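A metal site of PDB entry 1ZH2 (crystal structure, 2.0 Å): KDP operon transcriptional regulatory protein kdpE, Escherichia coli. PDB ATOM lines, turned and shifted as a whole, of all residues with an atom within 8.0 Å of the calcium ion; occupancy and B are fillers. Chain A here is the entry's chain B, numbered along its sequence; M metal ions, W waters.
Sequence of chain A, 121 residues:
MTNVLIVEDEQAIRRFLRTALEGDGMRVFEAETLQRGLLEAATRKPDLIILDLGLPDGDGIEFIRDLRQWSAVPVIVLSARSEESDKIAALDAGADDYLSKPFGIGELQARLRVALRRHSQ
Water W3 lies within hydrogen-bond range of OE1 of Glu 10, OE2 of Glu 8 and NZ of Lys 101.
The backbone carbonyl oxygen (O) of Val 7 is in hydrogen-bond range of the backbone NH (N) of Asp 52 (2.8 Å). The backbone NH of Glu 10 lies close to the side-chain carboxylate of Glu 8, 3.1 Å away. The side-chain carboxylate (OD1) of Asp 52 lies within salt-bridge range of the side-chain amino group (NZ) of Lys 101 (3.5 Å).
The calcium ion is bound by the backbone carbonyl oxygen (O) of Gly 54 (2.2 Å), the side-chain carboxylate (OD1) of Asp 9 (2.3 Å), the side-chain carboxylate (OD2) of Asp 52 (2.4 Å), water W1 (2.4 Å), water W2 (2.5 Å), water W3 (2.5 Å) and the side-chain carboxylate (OE1) of Glu 8 (2.5 Å).
Four residues have an atom within 4 Å of the calcium ion: Glu 8, Asp 9, Asp 52 and Gly 54.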
ATOM      1  N   VAL A   7     -26.490  -6.994  -9.497  1.00  0.00           N
ATOM      2  CA  VAL A   7     -27.310  -5.870  -9.950  1.00  0.00           C
ATOM      3  C   VAL A   7     -26.535  -4.596  -9.579  1.00  0.00           C
ATOM      4  O   VAL A   7     -26.444  -4.239  -8.371  1.00  0.00           O
ATOM      5  CB  VAL A   7     -28.695  -5.906  -9.284  1.00  0.00           C
ATOM      6  CG1 VAL A   7     -29.611  -4.746  -9.773  1.00  0.00           C
ATOM      7  CG2 VAL A   7     -29.391  -7.282  -9.618  1.00  0.00           C
ATOM      8  N   GLU A   8     -25.965  -3.934 -10.598  1.00  0.00           N
ATOM      9  CA  GLU A   8     -25.013  -2.820 -10.369  1.00  0.00           C
ATOM     10  C   GLU A   8     -24.835  -2.128 -11.710  1.00  0.00           C
ATOM     11  O   GLU A   8     -24.482  -2.776 -12.694  1.00  0.00           O
ATOM     12  CB  GLU A   8     -23.666  -3.380  -9.894  1.00  0.00           C
ATOM     13  CG  GLU A   8     -22.442  -2.431  -9.932  1.00  0.00           C
ATOM     14  CD  GLU A   8     -22.588  -1.260  -8.986  1.00  0.00           C
ATOM     15  OE1 GLU A   8     -23.433  -0.358  -9.254  1.00  0.00           O
ATOM     16  OE2 GLU A   8     -21.867  -1.211  -7.956  1.00  0.00           O
ATOM     17  N   ASP A   9     -25.140  -0.824 -11.764  1.00  0.00           N
ATOM     18  CA  ASP A   9     -24.939  -0.069 -13.008  1.00  0.00           C
ATOM     19  C   ASP A   9     -23.441   0.099 -13.293  1.00  0.00           C
ATOM     20  O   ASP A   9     -23.008   0.193 -14.452  1.00  0.00           O
ATOM     21  CB  ASP A   9     -25.535   1.298 -12.850  1.00  0.00           C
ATOM     22  CG  ASP A   9     -24.900   2.065 -11.696  1.00  0.00           C
ATOM     23  OD1 ASP A   9     -25.074   1.717 -10.490  1.00  0.00           O
ATOM     24  OD2 ASP A   9     -24.106   3.009 -11.963  1.00  0.00           O
ATOM     25  N   GLU A  10     -22.637   0.159 -12.230  1.00  0.00           N
ATOM     26  CA  GLU A  10     -21.254   0.616 -12.365  1.00  0.00           C
ATOM     27  C   GLU A  10     -20.370  -0.467 -12.969  1.00  0.00           C
ATOM     28  O   GLU A  10     -20.031  -1.473 -12.332  1.00  0.00           O
ATOM     29  CB  GLU A  10     -20.705   1.032 -11.011  1.00  0.00           C
ATOM     30  CG  GLU A  10     -19.279   1.544 -11.095  1.00  0.00           C
ATOM     31  CD  GLU A  10     -18.849   2.346  -9.868  1.00  0.00           C
ATOM     32  OE1 GLU A  10     -19.614   2.460  -8.882  1.00  0.00           O
ATOM     33  OE2 GLU A  10     -17.729   2.869  -9.887  1.00  0.00           O
ATOM     34  N   GLN A  11     -19.975  -0.253 -14.223  1.00  0.00           N
ATOM     35  CA  GLN A  11     -19.331  -1.334 -15.005  1.00  0.00           C
ATOM     36  C   GLN A  11     -18.065  -1.946 -14.371  1.00  0.00           C
ATOM     37  O   GLN A  11     -17.853  -3.167 -14.445  1.00  0.00           O
ATOM     38  CB  GLN A  11     -19.011  -0.838 -16.428  1.00  0.00           C
ATOM     39  CG  GLN A  11     -18.441  -1.954 -17.336  1.00  0.00           C
ATOM     40  CD  GLN A  11     -18.000  -1.435 -18.690  1.00  0.00           C
ATOM     41  OE1 GLN A  11     -16.859  -0.997 -18.844  1.00  0.00           O
ATOM     42  NE2 GLN A  11     -18.902  -1.473 -19.661  1.00  0.00           N
ATOM     43  N   ILE A  13     -17.183  -2.213 -11.157  1.00  0.00           N
ATOM     44  CA  ILE A  13     -17.575  -3.127 -10.079  1.00  0.00           C
ATOM     45  C   ILE A  13     -18.149  -4.443 -10.621  1.00  0.00           C
ATOM     46  O   ILE A  13     -17.758  -5.519 -10.181  1.00  0.00           O
ATOM     47  CB  ILE A  13     -18.544  -2.426  -9.116  1.00  0.00           C
ATOM     48  CG1 ILE A  13     -17.869  -1.147  -8.579  1.00  0.00           C
ATOM     49  CG2 ILE A  13     -18.958  -3.364  -7.994  1.00  0.00           C
ATOM     50  CD1 ILE A  13     -18.062  -0.876  -7.099  1.00  0.00           C
ATOM     51  N   GLU A  32     -27.924  -4.087 -15.123  1.00  0.00           N
ATOM     52  CA  GLU A  32     -27.422  -2.713 -14.885  1.00  0.00           C
ATOM     53  C   GLU A  32     -28.419  -1.731 -14.319  1.00  0.00           C
ATOM     54  O   GLU A  32     -28.080  -0.553 -14.098  1.00  0.00           O
ATOM     55  CB  GLU A  32     -26.881  -2.116 -16.208  1.00  0.00           C
ATOM     56  CG  GLU A  32     -25.726  -2.904 -16.771  1.00  0.00           C
ATOM     57  CD  GLU A  32     -25.352  -2.435 -18.173  1.00  0.00           C
ATOM     58  OE1 GLU A  32     -25.756  -1.329 -18.574  1.00  0.00           O
ATOM     59  OE2 GLU A  32     -24.677  -3.194 -18.887  1.00  0.00           O
ATOM     60  N   LEU A  51     -26.474  -6.939  -4.620  1.00  0.00           N
ATOM     61  CA  LEU A  51     -27.252  -5.785  -5.088  1.00  0.00           C
ATOM     62  C   LEU A  51     -26.517  -4.539  -4.680  1.00  0.00           C
ATOM     63  O   LEU A  51     -26.338  -4.285  -3.485  1.00  0.00           O
ATOM     64  CB  LEU A  51     -28.647  -5.774  -4.456  1.00  0.00           C
ATOM     65  CG  LEU A  51     -29.511  -4.500  -4.620  1.00  0.00           C
ATOM     66  CD1 LEU A  51     -30.009  -4.454  -6.054  1.00  0.00           C
ATOM     67  CD2 LEU A  51     -30.729  -4.549  -3.611  1.00  0.00           C
ATOM     68  N   ASP A  52     -26.080  -3.732  -5.659  1.00  0.00           N
ATOM     69  CA  ASP A  52     -25.632  -2.405  -5.283  1.00  0.00           C
ATOM     70  C   ASP A  52     -26.825  -1.477  -4.997  1.00  0.00           C
ATOM     71  O   ASP A  52     -27.810  -1.491  -5.720  1.00  0.00           O
ATOM     72  CB  ASP A  52     -24.720  -1.774  -6.332  1.00  0.00           C
ATOM     73  CG  ASP A  52     -24.268  -0.410  -5.878  1.00  0.00           C
ATOM     74  OD1 ASP A  52     -23.475  -0.348  -4.927  1.00  0.00           O
ATOM     75  OD2 ASP A  52     -24.750   0.620  -6.366  1.00  0.00           O
ATOM     76  N   LEU A  53     -26.750  -0.688  -3.929  1.00  0.00           N
ATOM     77  CA  LEU A  53     -27.924   0.136  -3.565  1.00  0.00           C
ATOM     78  C   LEU A  53     -28.065   1.439  -4.372  1.00  0.00           C
ATOM     79  O   LEU A  53     -29.125   2.054  -4.380  1.00  0.00           O
ATOM     80  CB  LEU A  53     -27.947   0.440  -2.061  1.00  0.00           C
ATOM     81  CG  LEU A  53     -28.159  -0.801  -1.162  1.00  0.00           C
ATOM     82  CD1 LEU A  53     -28.153  -0.399   0.314  1.00  0.00           C
ATOM     83  CD2 LEU A  53     -29.438  -1.537  -1.492  1.00  0.00           C
ATOM     84  N   GLY A  54     -27.009   1.868  -5.063  1.00  0.00           N
ATOM     85  CA  GLY A  54     -27.102   3.102  -5.832  1.00  0.00           C
ATOM     86  C   GLY A  54     -27.252   2.809  -7.296  1.00  0.00           C
ATOM     87  O   GLY A  54     -26.264   2.541  -7.987  1.00  0.00           O
ATOM     88  N   LEU A  55     -28.508   2.826  -7.747  1.00  0.00           N
ATOM     89  CA  LEU A  55     -28.892   2.421  -9.080  1.00  0.00           C
ATOM     90  C   LEU A  55     -29.634   3.594  -9.737  1.00  0.00           C
ATOM     91  O   LEU A  55     -30.277   4.372  -9.031  1.00  0.00           O
ATOM     92  CB  LEU A  55     -29.796   1.170  -9.028  1.00  0.00           C
ATOM     93  CG  LEU A  55     -29.180  -0.112  -8.456  1.00  0.00           C
ATOM     94  CD1 LEU A  55     -30.262  -1.180  -8.218  1.00  0.00           C
ATOM     95  CD2 LEU A  55     -28.020  -0.638  -9.349  1.00  0.00           C
ATOM     96  N   PRO A  56     -29.484   3.745 -11.056  1.00  0.00           N
ATOM     97  CA  PRO A  56     -29.972   4.957 -11.764  1.00  0.00           C
ATOM     98  C   PRO A  56     -31.473   5.081 -11.780  1.00  0.00           C
ATOM     99  O   PRO A  56     -31.988   6.194 -11.933  1.00  0.00           O
ATOM    100  CB  PRO A  56     -29.504   4.745 -13.222  1.00  0.00           C
ATOM    101  CG  PRO A  56     -29.035   3.328 -13.334  1.00  0.00           C
ATOM    102  CD  PRO A  56     -28.770   2.809 -11.945  1.00  0.00           C
ATOM    103  N   LEU A  78     -24.477  -3.936  -1.339  1.00  0.00           N
ATOM    104  CA  LEU A  78     -23.247  -3.138  -1.348  1.00  0.00           C
ATOM    105  C   LEU A  78     -23.654  -1.690  -1.328  1.00  0.00           C
ATOM    106  O   LEU A  78     -24.678  -1.354  -1.881  1.00  0.00           O
ATOM    107  CB  LEU A  78     -22.488  -3.393  -2.642  1.00  0.00           C
ATOM    108  CG  LEU A  78     -22.240  -4.875  -2.938  1.00  0.00           C
ATOM    109  CD1 LEU A  78     -21.496  -5.015  -4.330  1.00  0.00           C
ATOM    110  CD2 LEU A  78     -21.508  -5.600  -1.774  1.00  0.00           C
ATOM    111  N   SER A  79     -22.860  -0.811  -0.709  1.00  0.00           N
ATOM    112  CA  SER A  79     -23.175   0.616  -0.740  1.00  0.00           C
ATOM    113  C   SER A  79     -21.908   1.429  -0.627  1.00  0.00           C
ATOM    114  O   SER A  79     -20.929   1.003  -0.010  1.00  0.00           O
ATOM    115  CB  SER A  79     -24.094   1.020   0.412  1.00  0.00           C
ATOM    116  OG  SER A  79     -24.617   2.333   0.199  1.00  0.00           O
ATOM    117  N   ALA A  80     -21.940   2.615  -1.236  1.00  0.00           N
ATOM    118  CA  ALA A  80     -20.933   3.631  -0.968  1.00  0.00           C
ATOM    119  C   ALA A  80     -21.190   4.263   0.428  1.00  0.00           C
ATOM    120  O   ALA A  80     -20.265   4.773   1.051  1.00  0.00           O
ATOM    121  CB  ALA A  80     -20.950   4.681  -2.058  1.00  0.00           C
ATOM    122  N   LYS A 101     -18.476   0.260   0.819  1.00  0.00           N
ATOM    123  CA  LYS A 101     -17.230   0.371   0.060  1.00  0.00           C
ATOM    124  C   LYS A 101     -16.331   1.431   0.685  1.00  0.00           C
ATOM    125  O   LYS A 101     -16.798   2.454   1.114  1.00  0.00           O
ATOM    126  CB  LYS A 101     -17.533   0.753  -1.393  1.00  0.00           C
ATOM    127  CG  LYS A 101     -18.414  -0.288  -2.128  1.00  0.00           C
ATOM    128  CD  LYS A 101     -18.717   0.156  -3.567  1.00  0.00           C
ATOM    129  CE  LYS A 101     -19.933   1.032  -3.582  1.00  0.00           C
ATOM    130  NZ  LYS A 101     -20.466   1.414  -4.930  1.00  0.00           N
HETATM  131 CA    CA M   1     -24.173   1.871  -8.335  1.00  0.00          CA
HETATM  132  O   HOH W   1     -23.085   3.647  -9.625  1.00  0.00           O
HETATM  133  O   HOH W   2     -23.756   3.808  -6.863  1.00  0.00           O
HETATM  134  O   HOH W   3     -21.807   1.492  -7.642  1.00  0.00           O
